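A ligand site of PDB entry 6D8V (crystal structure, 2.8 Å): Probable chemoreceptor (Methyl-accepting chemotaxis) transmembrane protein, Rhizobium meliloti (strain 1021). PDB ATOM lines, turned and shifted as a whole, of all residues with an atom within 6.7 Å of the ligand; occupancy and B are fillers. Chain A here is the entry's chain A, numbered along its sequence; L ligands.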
ATOM      1  N   GLY A  70      -1.709 -20.916  22.821  1.00  0.00           N
ATOM      2  CA  GLY A  70      -3.025 -20.313  22.845  1.00  0.00           C
ATOM      3  C   GLY A  70      -4.013 -21.149  23.614  1.00  0.00           C
ATOM      4  O   GLY A  70      -3.819 -22.352  23.805  1.00  0.00           O
ATOM      5  N   TRP A  72      -8.361 -21.639  23.952  1.00  0.00           N
ATOM      6  CA  TRP A  72      -9.579 -21.329  23.209  1.00  0.00           C
ATOM      7  C   TRP A  72     -10.755 -22.097  23.785  1.00  0.00           C
ATOM      8  O   TRP A  72     -10.628 -22.928  24.701  1.00  0.00           O
ATOM      9  CB  TRP A  72      -9.394 -21.634  21.720  1.00  0.00           C
ATOM     10  CG  TRP A  72      -8.765 -22.966  21.471  1.00  0.00           C
ATOM     11  CD1 TRP A  72      -7.428 -23.232  21.345  1.00  0.00           C
ATOM     12  CD2 TRP A  72      -9.437 -24.215  21.318  1.00  0.00           C
ATOM     13  NE1 TRP A  72      -7.237 -24.565  21.114  1.00  0.00           N
ATOM     14  CE2 TRP A  72      -8.454 -25.189  21.084  1.00  0.00           C
ATOM     15  CE3 TRP A  72     -10.780 -24.609  21.332  1.00  0.00           C
ATOM     16  CZ2 TRP A  72      -8.761 -26.533  20.890  1.00  0.00           C
ATOM     17  CZ3 TRP A  72     -11.087 -25.936  21.135  1.00  0.00           C
ATOM     18  CH2 TRP A  72     -10.085 -26.877  20.915  1.00  0.00           C
ATOM     19  N   PHE A  73     -11.935 -21.799  23.235  1.00  0.00           N
ATOM     20  CA  PHE A  73     -13.165 -22.515  23.566  1.00  0.00           C
ATOM     21  C   PHE A  73     -14.152 -22.363  22.421  1.00  0.00           C
ATOM     22  O   PHE A  73     -14.571 -21.242  22.118  1.00  0.00           O
ATOM     23  CB  PHE A  73     -13.771 -22.009  24.869  1.00  0.00           C
ATOM     24  CG  PHE A  73     -15.195 -22.459  25.067  1.00  0.00           C
ATOM     25  CD1 PHE A  73     -15.480 -23.783  25.334  1.00  0.00           C
ATOM     26  CD2 PHE A  73     -16.245 -21.556  24.978  1.00  0.00           C
ATOM     27  CE1 PHE A  73     -16.780 -24.206  25.505  1.00  0.00           C
ATOM     28  CE2 PHE A  73     -17.552 -21.972  25.150  1.00  0.00           C
ATOM     29  CZ  PHE A  73     -17.824 -23.296  25.419  1.00  0.00           C
ATOM     30  N   ALA A  74     -14.535 -23.474  21.809  1.00  0.00           N
ATOM     31  CA  ALA A  74     -15.596 -23.501  20.815  1.00  0.00           C
ATOM     32  C   ALA A  74     -16.866 -24.037  21.463  1.00  0.00           C
ATOM     33  O   ALA A  74     -16.873 -25.145  22.004  1.00  0.00           O
ATOM     34  CB  ALA A  74     -15.210 -24.358  19.613  1.00  0.00           C
ATOM     35  N   PRO A 101     -14.138 -17.607  21.698  1.00  0.00           N
ATOM     36  CA  PRO A 101     -13.011 -16.815  22.195  1.00  0.00           C
ATOM     37  C   PRO A 101     -11.693 -17.528  21.970  1.00  0.00           C
ATOM     38  O   PRO A 101     -11.610 -18.760  21.986  1.00  0.00           O
ATOM     39  CB  PRO A 101     -13.293 -16.686  23.694  1.00  0.00           C
ATOM     40  CG  PRO A 101     -14.626 -17.334  23.939  1.00  0.00           C
ATOM     41  CD  PRO A 101     -14.875 -18.255  22.792  1.00  0.00           C
ATOM     42  N   TYR A 102     -10.640 -16.737  21.772  1.00  0.00           N
ATOM     43  CA  TYR A 102      -9.331 -17.324  21.484  1.00  0.00           C
ATOM     44  C   TYR A 102      -8.228 -16.362  21.922  1.00  0.00           C
ATOM     45  O   TYR A 102      -8.021 -15.330  21.293  1.00  0.00           O
ATOM     46  CB  TYR A 102      -9.203 -17.650  20.001  1.00  0.00           C
ATOM     47  CG  TYR A 102      -7.888 -18.290  19.631  1.00  0.00           C
ATOM     48  CD1 TYR A 102      -7.198 -19.075  20.552  1.00  0.00           C
ATOM     49  CD2 TYR A 102      -7.346 -18.123  18.370  1.00  0.00           C
ATOM     50  CE1 TYR A 102      -5.996 -19.668  20.216  1.00  0.00           C
ATOM     51  CE2 TYR A 102      -6.142 -18.712  18.025  1.00  0.00           C
ATOM     52  CZ  TYR A 102      -5.474 -19.478  18.950  1.00  0.00           C
ATOM     53  OH  TYR A 102      -4.277 -20.074  18.601  1.00  0.00           O
ATOM     54  N   SER A 104      -4.243 -15.962  22.061  1.00  0.00           N
ATOM     55  CA  SER A 104      -3.101 -16.492  21.323  1.00  0.00           C
ATOM     56  C   SER A 104      -1.950 -15.509  21.410  1.00  0.00           C
ATOM     57  O   SER A 104      -2.105 -14.373  21.886  1.00  0.00           O
ATOM     58  CB  SER A 104      -3.470 -16.746  19.855  1.00  0.00           C
ATOM     59  OG  SER A 104      -3.874 -15.541  19.230  1.00  0.00           O
ATOM     60  N   THR A 115     -10.634 -14.739  17.224  1.00  0.00           N
ATOM     61  CA  THR A 115     -11.876 -15.478  17.084  1.00  0.00           C
ATOM     62  C   THR A 115     -11.748 -16.347  15.845  1.00  0.00           C
ATOM     63  O   THR A 115     -11.012 -16.009  14.906  1.00  0.00           O
ATOM     64  CB  THR A 115     -13.095 -14.565  16.976  1.00  0.00           C
ATOM     65  OG1 THR A 115     -13.184 -13.744  18.150  1.00  0.00           O
ATOM     66  CG2 THR A 115     -14.366 -15.384  16.847  1.00  0.00           C
ATOM     67  N   PHE A 116     -12.451 -17.480  15.847  1.00  0.00           N
ATOM     68  CA  PHE A 116     -12.279 -18.495  14.818  1.00  0.00           C
ATOM     69  C   PHE A 116     -13.632 -19.063  14.426  1.00  0.00           C
ATOM     70  O   PHE A 116     -14.650 -18.816  15.078  1.00  0.00           O
ATOM     71  CB  PHE A 116     -11.343 -19.598  15.302  1.00  0.00           C
ATOM     72  CG  PHE A 116     -11.772 -20.243  16.599  1.00  0.00           C
ATOM     73  CD1 PHE A 116     -11.533 -19.608  17.812  1.00  0.00           C
ATOM     74  CD2 PHE A 116     -12.408 -21.467  16.598  1.00  0.00           C
ATOM     75  CE1 PHE A 116     -11.935 -20.199  19.004  1.00  0.00           C
ATOM     76  CE2 PHE A 116     -12.801 -22.061  17.779  1.00  0.00           C
ATOM     77  CZ  PHE A 116     -12.561 -21.423  18.983  1.00  0.00           C
ATOM     78  N   LYS A 117     -13.634 -19.819  13.328  1.00  0.00           N
ATOM     79  CA  LYS A 117     -14.850 -20.433  12.819  1.00  0.00           C
ATOM     80  C   LYS A 117     -15.142 -21.737  13.542  1.00  0.00           C
ATOM     81  O   LYS A 117     -14.227 -22.487  13.915  1.00  0.00           O
ATOM     82  CB  LYS A 117     -14.757 -20.686  11.315  1.00  0.00           C
ATOM     83  CG  LYS A 117     -15.905 -21.538  10.772  1.00  0.00           C
ATOM     84  CD  LYS A 117     -15.750 -21.897   9.302  1.00  0.00           C
ATOM     85  CE  LYS A 117     -16.916 -22.773   8.844  1.00  0.00           C
ATOM     86  NZ  LYS A 117     -16.943 -22.986   7.372  1.00  0.00           N
ATOM     87  N   ALA A 122     -13.921 -30.410  12.284  1.00  0.00           N
ATOM     88  CA  ALA A 122     -12.471 -30.314  12.368  1.00  0.00           C
ATOM     89  C   ALA A 122     -11.937 -31.183  13.495  1.00  0.00           C
ATOM     90  O   ALA A 122     -12.619 -31.440  14.492  1.00  0.00           O
ATOM     91  CB  ALA A 122     -12.041 -28.864  12.584  1.00  0.00           C
ATOM     92  N   TRP A 124      -9.847 -30.661  15.852  1.00  0.00           N
ATOM     93  CA  TRP A 124      -9.710 -30.075  17.185  1.00  0.00           C
ATOM     94  C   TRP A 124     -11.028 -30.043  17.935  1.00  0.00           C
ATOM     95  O   TRP A 124     -11.015 -29.980  19.170  1.00  0.00           O
ATOM     96  CB  TRP A 124      -9.121 -28.668  17.084  1.00  0.00           C
ATOM     97  CG  TRP A 124      -9.862 -27.807  16.109  1.00  0.00           C
ATOM     98  CD1 TRP A 124      -9.562 -27.616  14.793  1.00  0.00           C
ATOM     99  CD2 TRP A 124     -11.050 -27.058  16.364  1.00  0.00           C
ATOM    100  NE1 TRP A 124     -10.480 -26.766  14.219  1.00  0.00           N
ATOM    101  CE2 TRP A 124     -11.398 -26.404  15.162  1.00  0.00           C
ATOM    102  CE3 TRP A 124     -11.834 -26.847  17.506  1.00  0.00           C
ATOM    103  CZ2 TRP A 124     -12.511 -25.573  15.071  1.00  0.00           C
ATOM    104  CZ3 TRP A 124     -12.938 -26.018  17.404  1.00  0.00           C
ATOM    105  CH2 TRP A 124     -13.270 -25.391  16.194  1.00  0.00           C
ATOM    106  N   TYR A 125     -12.157 -30.085  17.226  1.00  0.00           N
ATOM    107  CA  TYR A 125     -13.464 -30.198  17.861  1.00  0.00           C
ATOM    108  C   TYR A 125     -14.033 -31.615  17.822  1.00  0.00           C
ATOM    109  O   TYR A 125     -14.528 -32.107  18.843  1.00  0.00           O
ATOM    110  CB  TYR A 125     -14.459 -29.237  17.211  1.00  0.00           C
ATOM    111  CG  TYR A 125     -15.663 -28.941  18.071  1.00  0.00           C
ATOM    112  CD1 TYR A 125     -16.725 -29.826  18.149  1.00  0.00           C
ATOM    113  CD2 TYR A 125     -15.730 -27.777  18.825  1.00  0.00           C
ATOM    114  CE1 TYR A 125     -17.828 -29.555  18.949  1.00  0.00           C
ATOM    115  CE2 TYR A 125     -16.825 -27.496  19.620  1.00  0.00           C
ATOM    116  CZ  TYR A 125     -17.869 -28.386  19.676  1.00  0.00           C
ATOM    117  OH  TYR A 125     -18.957 -28.112  20.469  1.00  0.00           O
ATOM    118  N   TYR A 140      -1.874 -28.969  12.297  1.00  0.00           N
ATOM    119  CA  TYR A 140      -2.710 -28.240  11.359  1.00  0.00           C
ATOM    120  C   TYR A 140      -2.371 -26.762  11.455  1.00  0.00           C
ATOM    121  O   TYR A 140      -1.859 -26.278  12.467  1.00  0.00           O
ATOM    122  CB  TYR A 140      -4.207 -28.451  11.634  1.00  0.00           C
ATOM    123  CG  TYR A 140      -4.691 -27.767  12.900  1.00  0.00           C
ATOM    124  CD1 TYR A 140      -4.479 -28.340  14.145  1.00  0.00           C
ATOM    125  CD2 TYR A 140      -5.332 -26.538  12.842  1.00  0.00           C
ATOM    126  CE1 TYR A 140      -4.889 -27.717  15.302  1.00  0.00           C
ATOM    127  CE2 TYR A 140      -5.748 -25.905  13.991  1.00  0.00           C
ATOM    128  CZ  TYR A 140      -5.534 -26.501  15.217  1.00  0.00           C
ATOM    129  OH  TYR A 140      -5.951 -25.871  16.376  1.00  0.00           O
ATOM    130  N   LEU A 141      -2.665 -26.055  10.365  1.00  0.00           N
ATOM    131  CA  LEU A 141      -2.454 -24.616  10.312  1.00  0.00           C
ATOM    132  C   LEU A 141      -3.630 -23.903  10.952  1.00  0.00           C
ATOM    133  O   LEU A 141      -4.760 -23.992  10.462  1.00  0.00           O
ATOM    134  CB  LEU A 141      -2.271 -24.160   8.862  1.00  0.00           C
ATOM    135  CG  LEU A 141      -2.362 -22.652   8.655  1.00  0.00           C
ATOM    136  CD1 LEU A 141      -1.240 -21.950   9.408  1.00  0.00           C
ATOM    137  CD2 LEU A 141      -2.345 -22.243   7.177  1.00  0.00           C
ATOM    138  N   ALA A 142      -3.367 -23.165  12.024  1.00  0.00           N
ATOM    139  CA  ALA A 142      -4.394 -22.458  12.777  1.00  0.00           C
ATOM    140  C   ALA A 142      -4.898 -21.219  12.034  1.00  0.00           C
ATOM    141  O   ALA A 142      -4.130 -20.521  11.379  1.00  0.00           O
ATOM    142  CB  ALA A 142      -3.866 -22.064  14.155  1.00  0.00           C
ATOM    143  N   GLU A 143      -6.210 -20.946  12.186  1.00  0.00           N
ATOM    144  CA  GLU A 143      -6.893 -19.837  11.523  1.00  0.00           C
ATOM    145  C   GLU A 143      -6.884 -18.550  12.331  1.00  0.00           C
ATOM    146  O   GLU A 143      -6.537 -17.488  11.817  1.00  0.00           O
ATOM    147  CB  GLU A 143      -8.356 -20.210  11.218  1.00  0.00           C
ATOM    148  CG  GLU A 143      -9.249 -18.980  11.021  1.00  0.00           C
ATOM    149  CD  GLU A 143     -10.739 -19.320  11.004  1.00  0.00           C
ATOM    150  OE1 GLU A 143     -11.065 -20.515  10.873  1.00  0.00           O
ATOM    151  OE2 GLU A 143     -11.562 -18.386  11.127  1.00  0.00           O
ATOM    152  N   GLY A 144      -7.301 -18.604  13.596  1.00  0.00           N
ATOM    153  CA  GLY A 144      -7.499 -17.393  14.361  1.00  0.00           C
ATOM    154  C   GLY A 144      -6.241 -16.728  14.862  1.00  0.00           C
ATOM    155  O   GLY A 144      -6.329 -15.667  15.480  1.00  0.00           O
ATOM    156  N   THR A 145      -5.078 -17.321  14.606  1.00  0.00           N
ATOM    157  CA  THR A 145      -3.830 -16.740  15.086  1.00  0.00           C
ATOM    158  C   THR A 145      -3.525 -15.458  14.325  1.00  0.00           C
ATOM    159  O   THR A 145      -3.896 -15.286  13.160  1.00  0.00           O
ATOM    160  CB  THR A 145      -2.685 -17.744  14.927  1.00  0.00           C
ATOM    161  OG1 THR A 145      -2.572 -18.140  13.556  1.00  0.00           O
ATOM    162  CG2 THR A 145      -2.940 -18.971  15.779  1.00  0.00           C
ATOM    163  N   MET A 151       0.317 -25.654  14.444  1.00  0.00           N
ATOM    164  CA  MET A 151       0.231 -26.034  15.849  1.00  0.00           C
ATOM    165  C   MET A 151      -0.534 -27.355  15.968  1.00  0.00           C
ATOM    166  O   MET A 151      -1.240 -27.774  15.050  1.00  0.00           O
ATOM    167  CB  MET A 151      -0.485 -24.967  16.665  1.00  0.00           C
ATOM    168  CG  MET A 151      -1.923 -24.783  16.191  1.00  0.00           C
ATOM    169  SD  MET A 151      -2.836 -23.524  17.062  1.00  0.00           S
ATOM    170  CE  MET A 151      -1.792 -22.086  16.817  1.00  0.00           C
ATOM    171  N   SER A 153      -3.249 -29.226  18.859  1.00  0.00           N
ATOM    172  CA  SER A 153      -4.206 -28.769  19.863  1.00  0.00           C
ATOM    173  C   SER A 153      -4.643 -29.897  20.781  1.00  0.00           C
ATOM    174  O   SER A 153      -5.012 -30.978  20.321  1.00  0.00           O
ATOM    175  CB  SER A 153      -5.413 -28.126  19.199  1.00  0.00           C
ATOM    176  OG  SER A 153      -5.067 -26.874  18.657  1.00  0.00           O
ATOM    177  N   ASP A 171      -3.031 -24.931  22.816  1.00  0.00           N
ATOM    178  CA  ASP A 171      -2.243 -25.122  21.597  1.00  0.00           C
ATOM    179  C   ASP A 171      -0.760 -25.198  21.880  1.00  0.00           C
ATOM    180  O   ASP A 171      -0.249 -24.520  22.770  1.00  0.00           O
ATOM    181  CB  ASP A 171      -2.490 -24.003  20.565  1.00  0.00           C
ATOM    182  CG  ASP A 171      -3.939 -23.882  20.184  1.00  0.00           C
ATOM    183  OD1 ASP A 171      -4.679 -24.892  20.280  1.00  0.00           O
ATOM    184  OD2 ASP A 171      -4.338 -22.764  19.786  1.00  0.00           O
HETATM  185  N1  LIG L   1      -7.787 -22.563  17.234  1.00  0.00           N
HETATM  186  C1  LIG L   1      -8.268 -23.592  17.882  1.00  0.00           C
HETATM  187  C2  LIG L   1      -7.870 -23.047  15.795  1.00  0.00           C
HETATM  188  C3  LIG L   1      -9.315 -23.704  15.766  1.00  0.00           C
HETATM  189  C4  LIG L   1      -9.481 -24.158  16.941  1.00  0.00           C
HETATM  190  C5  LIG L   1      -8.620 -21.372  17.481  1.00  0.00           C
HETATM  191  C6  LIG L   1      -6.384 -22.325  17.632  1.00  0.00           C
HETATM  192  C7  LIG L   1      -7.722 -22.046  14.773  1.00  0.00           C
HETATM  193  O1  LIG L   1      -8.111 -22.307  13.600  1.00  0.00           O
HETATM  194  O2  LIG L   1      -7.188 -20.927  15.011  1.00  0.00           O
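N of Lys 117 is in hydrogen-bond range of OE2 of Glu 143 (3.3 Å).
The side-chain carboxylate of Asp 171 lies within hydrogen-bond range of the side-chain hydroxyl of Tyr 102, 2.9 Å away.
The indole nitrogen of Trp 72 lies within hydrogen-bond range of the side-chain carboxylate of Asp 171 (2.7 Å).
OD1 of Asp 171 lies within hydrogen-bond range of OG of Ser 153.
The backbone NH (N) of Asp 171 sits at hydrogen-bond distance from the backbone carbonyl oxygen (O) of Gly 70 (2.9 Å).
The backbone NH (N) of Met 151 sits at hydrogen-bond distance from the backbone carbonyl oxygen (O) of Tyr 140.
The side-chain hydroxyl (OG) of Ser 153 is in hydrogen-bond range of the side-chain hydroxyl (OH) of Tyr 140 (2.6 Å).
Merely in contact with the ligand: Trp 72 (3.5 Å), Tyr 102 (3.2 Å), Phe 116 (3.4 Å), Trp 124 (3.3 Å), Tyr 140 (3.5 Å), Ala 142 (3.6 Å), Met 151 (3.8 Å) and Asp 171 (3.0 Å).
Hydrophobic or aromatic side chains within 4 Å of the ligand: Trp 72, Tyr 102, Phe 116, Trp 124, Tyr 140, Ala 142 and Met 151.
The nearest printed residue that does not touch the ligand is Thr 145 (4.2 Å).
The backbone NH (N) of Gly 144 is in hydrogen-bond range of an oxygen (O2) of the ligand (2.7 Å).
An oxygen (O1) of the ligand is in hydrogen-bond range of the backbone NH of Glu 143 (2.7 Å).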
